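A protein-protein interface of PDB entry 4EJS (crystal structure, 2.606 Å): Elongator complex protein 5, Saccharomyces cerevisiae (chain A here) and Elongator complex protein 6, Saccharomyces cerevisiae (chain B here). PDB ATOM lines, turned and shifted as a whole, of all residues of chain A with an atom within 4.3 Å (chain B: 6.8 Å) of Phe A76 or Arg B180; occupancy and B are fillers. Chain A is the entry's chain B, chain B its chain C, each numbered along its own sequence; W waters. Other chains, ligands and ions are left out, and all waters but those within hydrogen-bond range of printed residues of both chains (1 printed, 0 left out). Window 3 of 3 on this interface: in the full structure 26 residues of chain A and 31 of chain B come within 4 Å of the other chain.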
ATOM      1  N   TYR A  61     -36.074  26.156 -24.241  1.00  0.00           N
ATOM      2  CA  TYR A  61     -35.331  25.007 -24.732  1.00  0.00           C
ATOM      3  C   TYR A  61     -34.032  24.796 -23.958  1.00  0.00           C
ATOM      4  O   TYR A  61     -33.161  25.664 -23.960  1.00  0.00           O
ATOM      5  CB  TYR A  61     -35.021  25.217 -26.212  1.00  0.00           C
ATOM      6  CG  TYR A  61     -34.556  23.968 -26.895  1.00  0.00           C
ATOM      7  CD1 TYR A  61     -35.445  23.167 -27.600  1.00  0.00           C
ATOM      8  CD2 TYR A  61     -33.232  23.582 -26.832  1.00  0.00           C
ATOM      9  CE1 TYR A  61     -35.025  22.015 -28.233  1.00  0.00           C
ATOM     10  CE2 TYR A  61     -32.800  22.436 -27.453  1.00  0.00           C
ATOM     11  CZ  TYR A  61     -33.697  21.653 -28.155  1.00  0.00           C
ATOM     12  OH  TYR A  61     -33.248  20.501 -28.768  1.00  0.00           O
ATOM     13  N   SER A  63     -30.595  22.834 -23.569  1.00  0.00           N
ATOM     14  CA  SER A  63     -29.716  22.092 -24.462  1.00  0.00           C
ATOM     15  C   SER A  63     -28.436  21.547 -23.841  1.00  0.00           C
ATOM     16  O   SER A  63     -27.626  22.292 -23.284  1.00  0.00           O
ATOM     17  CB  SER A  63     -29.360  22.953 -25.663  1.00  0.00           C
ATOM     18  OG  SER A  63     -28.236  22.414 -26.320  1.00  0.00           O
ATOM     19  N   THR A  66     -27.677  20.064 -28.212  1.00  0.00           N
ATOM     20  CA  THR A  66     -28.268  20.769 -29.354  1.00  0.00           C
ATOM     21  C   THR A  66     -27.526  22.075 -29.570  1.00  0.00           C
ATOM     22  O   THR A  66     -27.652  23.033 -28.816  1.00  0.00           O
ATOM     23  CB  THR A  66     -29.770  21.042 -29.168  1.00  0.00           C
ATOM     24  OG1 THR A  66     -30.431  19.807 -28.890  1.00  0.00           O
ATOM     25  CG2 THR A  66     -30.395  21.682 -30.441  1.00  0.00           C
ATOM     26  N   VAL A  67     -26.741  22.099 -30.625  1.00  0.00           N
ATOM     27  CA  VAL A  67     -25.772  23.153 -30.828  1.00  0.00           C
ATOM     28  C   VAL A  67     -26.352  24.199 -31.802  1.00  0.00           C
ATOM     29  O   VAL A  67     -25.952  25.352 -31.793  1.00  0.00           O
ATOM     30  CB  VAL A  67     -24.424  22.498 -31.246  1.00  0.00           C
ATOM     31  CG1 VAL A  67     -24.109  22.667 -32.731  1.00  0.00           C
ATOM     32  CG2 VAL A  67     -23.294  22.928 -30.327  1.00  0.00           C
ATOM     33  N   LYS A  69     -29.552  26.383 -32.377  1.00  0.00           N
ATOM     34  CA  LYS A  69     -30.755  26.901 -31.730  1.00  0.00           C
ATOM     35  C   LYS A  69     -31.941  26.772 -32.666  1.00  0.00           C
ATOM     36  O   LYS A  69     -31.946  27.323 -33.772  1.00  0.00           O
ATOM     37  CB  LYS A  69     -30.537  28.356 -31.255  1.00  0.00           C
ATOM     38  CG  LYS A  69     -31.760  29.053 -30.631  1.00  0.00           C
ATOM     39  CD  LYS A  69     -31.451  30.495 -30.155  1.00  0.00           C
ATOM     40  CE  LYS A  69     -32.741  31.235 -29.716  1.00  0.00           C
ATOM     41  NZ  LYS A  69     -32.577  32.404 -28.768  1.00  0.00           N
ATOM     42  N   PRO A  70     -32.949  26.003 -32.238  1.00  0.00           N
ATOM     43  CA  PRO A  70     -34.187  25.787 -32.996  1.00  0.00           C
ATOM     44  C   PRO A  70     -34.907  27.103 -33.238  1.00  0.00           C
ATOM     45  O   PRO A  70     -34.899  27.985 -32.376  1.00  0.00           O
ATOM     46  CB  PRO A  70     -35.022  24.913 -32.060  1.00  0.00           C
ATOM     47  CG  PRO A  70     -34.015  24.269 -31.144  1.00  0.00           C
ATOM     48  CD  PRO A  70     -32.932  25.268 -30.962  1.00  0.00           C
ATOM     49  N   CYS A  73     -38.074  28.175 -30.637  1.00  0.00           N
ATOM     50  CA  CYS A  73     -37.951  28.467 -29.211  1.00  0.00           C
ATOM     51  C   CYS A  73     -37.849  29.967 -28.937  1.00  0.00           C
ATOM     52  O   CYS A  73     -37.392  30.745 -29.775  1.00  0.00           O
ATOM     53  CB  CYS A  73     -36.786  27.689 -28.566  1.00  0.00           C
ATOM     54  SG  CYS A  73     -35.134  28.361 -28.857  1.00  0.00           S
ATOM     55  N   GLN A  75     -36.784  31.012 -25.562  1.00  0.00           N
ATOM     56  CA  GLN A  75     -35.567  31.007 -24.752  1.00  0.00           C
ATOM     57  C   GLN A  75     -34.723  29.785 -25.087  1.00  0.00           C
ATOM     58  O   GLN A  75     -35.237  28.698 -25.371  1.00  0.00           O
ATOM     59  CB  GLN A  75     -35.884  30.992 -23.258  1.00  0.00           C
ATOM     60  CG  GLN A  75     -36.725  32.149 -22.789  1.00  0.00           C
ATOM     61  CD  GLN A  75     -36.027  33.480 -22.968  1.00  0.00           C
ATOM     62  OE1 GLN A  75     -36.667  34.534 -22.908  1.00  0.00           O
ATOM     63  NE2 GLN A  75     -34.704  33.444 -23.188  1.00  0.00           N
ATOM     64  N   PHE A  76     -33.416  29.959 -25.048  1.00  0.00           N
ATOM     65  CA  PHE A  76     -32.532  28.846 -25.299  1.00  0.00           C
ATOM     66  C   PHE A  76     -31.475  28.850 -24.215  1.00  0.00           C
ATOM     67  O   PHE A  76     -30.721  29.808 -24.101  1.00  0.00           O
ATOM     68  CB  PHE A  76     -31.891  28.982 -26.684  1.00  0.00           C
ATOM     69  CG  PHE A  76     -30.965  27.855 -27.039  1.00  0.00           C
ATOM     70  CD1 PHE A  76     -31.450  26.714 -27.675  1.00  0.00           C
ATOM     71  CD2 PHE A  76     -29.607  27.929 -26.744  1.00  0.00           C
ATOM     72  CE1 PHE A  76     -30.597  25.664 -28.021  1.00  0.00           C
ATOM     73  CE2 PHE A  76     -28.745  26.878 -27.084  1.00  0.00           C
ATOM     74  CZ  PHE A  76     -29.246  25.746 -27.720  1.00  0.00           C
ATOM     75  N   ILE A  77     -31.429  27.786 -23.417  1.00  0.00           N
ATOM     76  CA  ILE A  77     -30.395  27.637 -22.388  1.00  0.00           C
ATOM     77  C   ILE A  77     -29.348  26.586 -22.762  1.00  0.00           C
ATOM     78  O   ILE A  77     -29.673  25.412 -22.936  1.00  0.00           O
ATOM     79  CB  ILE A  77     -31.009  27.271 -21.028  1.00  0.00           C
ATOM     80  CG1 ILE A  77     -32.024  28.331 -20.619  1.00  0.00           C
ATOM     81  CG2 ILE A  77     -29.921  27.101 -19.960  1.00  0.00           C
ATOM     82  CD1 ILE A  77     -33.005  27.848 -19.597  1.00  0.00           C
ATOM     83  N   ASP A  78     -28.099  27.021 -22.906  1.00  0.00           N
ATOM     84  CA  ASP A  78     -26.993  26.092 -23.046  1.00  0.00           C
ATOM     85  C   ASP A  78     -26.579  25.609 -21.653  1.00  0.00           C
ATOM     86  O   ASP A  78     -25.970  26.353 -20.880  1.00  0.00           O
ATOM     87  CB  ASP A  78     -25.796  26.706 -23.807  1.00  0.00           C
ATOM     88  CG  ASP A  78     -24.502  25.847 -23.685  1.00  0.00           C
ATOM     89  OD1 ASP A  78     -24.568  24.621 -23.412  1.00  0.00           O
ATOM     90  OD2 ASP A  78     -23.401  26.400 -23.851  1.00  0.00           O
ATOM     91  N   SER B  32     -24.665  27.937 -38.391  1.00  0.00           N
ATOM     92  CA  SER B  32     -24.896  26.503 -38.514  1.00  0.00           C
ATOM     93  C   SER B  32     -23.657  25.721 -38.116  1.00  0.00           C
ATOM     94  O   SER B  32     -22.530  26.162 -38.324  1.00  0.00           O
ATOM     95  CB  SER B  32     -25.334  26.111 -39.921  1.00  0.00           C
ATOM     96  OG  SER B  32     -24.214  25.879 -40.749  1.00  0.00           O
ATOM     97  N   HIS B  33     -23.893  24.556 -37.529  1.00  0.00           N
ATOM     98  CA  HIS B  33     -22.836  23.662 -37.091  1.00  0.00           C
ATOM     99  C   HIS B  33     -23.183  22.232 -37.490  1.00  0.00           C
ATOM    100  O   HIS B  33     -24.237  21.716 -37.122  1.00  0.00           O
ATOM    101  CB  HIS B  33     -22.670  23.741 -35.575  1.00  0.00           C
ATOM    102  CG  HIS B  33     -22.514  25.134 -35.058  1.00  0.00           C
ATOM    103  ND1 HIS B  33     -21.369  25.874 -35.256  1.00  0.00           N
ATOM    104  CD2 HIS B  33     -23.362  25.927 -34.358  1.00  0.00           C
ATOM    105  CE1 HIS B  33     -21.516  27.060 -34.695  1.00  0.00           C
ATOM    106  NE2 HIS B  33     -22.718  27.120 -34.147  1.00  0.00           N
ATOM    107  N   ILE B 175     -16.191  18.311 -26.542  1.00  0.00           N
ATOM    108  CA  ILE B 175     -16.809  18.082 -27.853  1.00  0.00           C
ATOM    109  C   ILE B 175     -17.852  19.133 -28.245  1.00  0.00           C
ATOM    110  O   ILE B 175     -17.744  19.760 -29.290  1.00  0.00           O
ATOM    111  CB  ILE B 175     -17.477  16.699 -27.981  1.00  0.00           C
ATOM    112  CG1 ILE B 175     -16.453  15.571 -27.816  1.00  0.00           C
ATOM    113  CG2 ILE B 175     -18.245  16.625 -29.328  1.00  0.00           C
ATOM    114  CD1 ILE B 175     -15.245  15.695 -28.714  1.00  0.00           C
ATOM    115  N   THR B 176     -18.875  19.300 -27.418  1.00  0.00           N
ATOM    116  CA  THR B 176     -19.955  20.233 -27.717  1.00  0.00           C
ATOM    117  C   THR B 176     -19.460  21.681 -27.827  1.00  0.00           C
ATOM    118  O   THR B 176     -19.834  22.380 -28.765  1.00  0.00           O
ATOM    119  CB  THR B 176     -21.106  20.070 -26.713  1.00  0.00           C
ATOM    120  OG1 THR B 176     -21.576  18.722 -26.778  1.00  0.00           O
ATOM    121  CG2 THR B 176     -22.248  20.974 -27.036  1.00  0.00           C
ATOM    122  N   PRO B 177     -18.598  22.138 -26.891  1.00  0.00           N
ATOM    123  CA  PRO B 177     -18.052  23.488 -27.099  1.00  0.00           C
ATOM    124  C   PRO B 177     -17.230  23.620 -28.392  1.00  0.00           C
ATOM    125  O   PRO B 177     -17.276  24.671 -29.052  1.00  0.00           O
ATOM    126  CB  PRO B 177     -17.154  23.703 -25.882  1.00  0.00           C
ATOM    127  CG  PRO B 177     -17.683  22.789 -24.852  1.00  0.00           C
ATOM    128  CD  PRO B 177     -18.288  21.613 -25.545  1.00  0.00           C
ATOM    129  N   LEU B 178     -16.481  22.576 -28.745  1.00  0.00           N
ATOM    130  CA  LEU B 178     -15.703  22.601 -29.983  1.00  0.00           C
ATOM    131  C   LEU B 178     -16.600  22.708 -31.211  1.00  0.00           C
ATOM    132  O   LEU B 178     -16.335  23.499 -32.117  1.00  0.00           O
ATOM    133  CB  LEU B 178     -14.818  21.364 -30.112  1.00  0.00           C
ATOM    134  CG  LEU B 178     -14.042  21.369 -31.422  1.00  0.00           C
ATOM    135  CD1 LEU B 178     -13.189  22.632 -31.546  1.00  0.00           C
ATOM    136  CD2 LEU B 178     -13.199  20.130 -31.541  1.00  0.00           C
ATOM    137  N   LEU B 179     -17.668  21.917 -31.236  1.00  0.00           N
ATOM    138  CA  LEU B 179     -18.617  21.959 -32.342  1.00  0.00           C
ATOM    139  C   LEU B 179     -19.269  23.331 -32.519  1.00  0.00           C
ATOM    140  O   LEU B 179     -19.592  23.720 -33.636  1.00  0.00           O
ATOM    141  CB  LEU B 179     -19.686  20.881 -32.170  1.00  0.00           C
ATOM    142  CG  LEU B 179     -20.752  20.840 -33.255  1.00  0.00           C
ATOM    143  CD1 LEU B 179     -20.131  20.578 -34.631  1.00  0.00           C
ATOM    144  CD2 LEU B 179     -21.788  19.784 -32.916  1.00  0.00           C
ATOM    145  N   ARG B 180     -19.461  24.043 -31.411  1.00  0.00           N
ATOM    146  CA  ARG B 180     -19.988  25.415 -31.399  1.00  0.00           C
ATOM    147  C   ARG B 180     -19.093  26.467 -32.050  1.00  0.00           C
ATOM    148  O   ARG B 180     -19.578  27.504 -32.493  1.00  0.00           O
ATOM    149  CB  ARG B 180     -20.259  25.864 -29.965  1.00  0.00           C
ATOM    150  CG  ARG B 180     -21.631  25.532 -29.514  1.00  0.00           C
ATOM    151  CD  ARG B 180     -21.994  26.216 -28.224  1.00  0.00           C
ATOM    152  NE  ARG B 180     -23.438  26.121 -28.054  1.00  0.00           N
ATOM    153  CZ  ARG B 180     -24.053  25.138 -27.402  1.00  0.00           C
ATOM    154  NH1 ARG B 180     -23.340  24.177 -26.819  1.00  0.00           N
ATOM    155  NH2 ARG B 180     -25.381  25.127 -27.329  1.00  0.00           N
ATOM    156  N   GLN B 181     -17.791  26.210 -32.087  1.00  0.00           N
ATOM    157  CA  GLN B 181     -16.842  27.169 -32.629  1.00  0.00           C
ATOM    158  C   GLN B 181     -16.464  26.899 -34.094  1.00  0.00           C
ATOM    159  O   GLN B 181     -15.665  27.629 -34.682  1.00  0.00           O
ATOM    160  CB  GLN B 181     -15.575  27.167 -31.789  1.00  0.00           C
ATOM    161  CG  GLN B 181     -15.820  27.411 -30.349  1.00  0.00           C
ATOM    162  CD  GLN B 181     -14.604  27.109 -29.525  1.00  0.00           C
ATOM    163  OE1 GLN B 181     -13.479  27.182 -30.015  1.00  0.00           O
ATOM    164  NE2 GLN B 181     -14.817  26.756 -28.266  1.00  0.00           N
ATOM    165  N   CYS B 182     -17.008  25.848 -34.686  1.00  0.00           N
ATOM    166  CA  CYS B 182     -16.713  25.620 -36.086  1.00  0.00           C
ATOM    167  C   CYS B 182     -17.919  25.253 -36.929  1.00  0.00           C
ATOM    168  O   CYS B 182     -18.945  24.804 -36.421  1.00  0.00           O
ATOM    169  CB  CYS B 182     -15.577  24.608 -36.270  1.00  0.00           C
ATOM    170  SG  CYS B 182     -15.810  23.045 -35.430  1.00  0.00           S
ATOM    171  N   LYS B 183     -17.765  25.468 -38.231  1.00  0.00           N
ATOM    172  CA  LYS B 183     -18.804  25.199 -39.207  1.00  0.00           C
ATOM    173  C   LYS B 183     -19.031  23.703 -39.421  1.00  0.00           C
ATOM    174  O   LYS B 183     -20.175  23.240 -39.407  1.00  0.00           O
ATOM    175  CB  LYS B 183     -18.461  25.893 -40.529  1.00  0.00           C
ATOM    176  CG  LYS B 183     -18.549  27.416 -40.452  1.00  0.00           C
ATOM    177  CD  LYS B 183     -19.975  27.846 -40.146  1.00  0.00           C
ATOM    178  CE  LYS B 183     -20.197  29.321 -40.429  1.00  0.00           C
ATOM    179  NZ  LYS B 183     -21.607  29.713 -40.150  1.00  0.00           N
HETATM  180  O   HOH W   1     -25.892  23.251 -25.708  1.00  0.00           O
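OD1 of Asp A78 is in salt-bridge range of NH1 of Arg B180 (3.6 Å).
O of Thr A66 lies within hydrogen-bond range of NH2 of Arg B180 (3.4 Å).
The backbone carbonyl oxygen (O) of Leu B179 lies within hydrogen-bond range of a ring nitrogen (ND1) of His B33 (3.2 Å).
O of Thr A66 lies within hydrogen-bond range of OG of Ser A63 (2.6 Å).
OH of Tyr A61 sits at hydrogen-bond distance from OG1 of Thr A66 (2.9 Å).
A ring nitrogen (ND1) of His B33 is in hydrogen-bond range of the backbone carbonyl oxygen (O) of Cys B182 (2.9 Å).
Val A67 touches His B33.
Thr B176 touches Val A67.
Leu B179 touches Val A67.
Val A67 touches Arg B180 (CG2 to CG, 3.2 Å).
Arg B180 touches Phe A76.
Of the printed residues of chain B, Val A67 touches His B33, Thr B176, Leu B179 and Arg B180.
Gln A75 touches none of the printed residues of chain B.
Of chain B, only Arg B180 comes within 4 Å of Phe A76.
Of the printed residues of chain B, Asp A78 touches Arg B180.
Printed residues of chain A within 4 Å of His B33: Val A67.
Printed residues of chain A within 4 Å of Leu B179: Val A67 (3.7 Å).
Of the 11 printed residues of chain A, 4 touch a printed residue of chain B.
Printed residues of chain A that touch a printed residue of chain B: Thr A66, Val A67, Phe A76 and Asp A78.
Along chain A the printed residues that touch a printed residue of chain B span positions 66 to 78.
Of the 11 printed residues of chain B, 4 touch a printed residue of chain A.
Hydrophobic or aromatic side chains of chain B that line the printed part of chain A: His B33 and Leu B179.
Among the printed residues, Asp or Glu carboxylates within 4 Å of a Lys or Arg side-chain nitrogen of the other chain: Asp A78 with Arg B180 (3.6 Å).
Water W1 lies within hydrogen-bond range of NH2 of Arg B180 (2.5 Å), OG of Ser A63 (2.6 Å) and OD1 of Asp A78 (3.0 Å).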
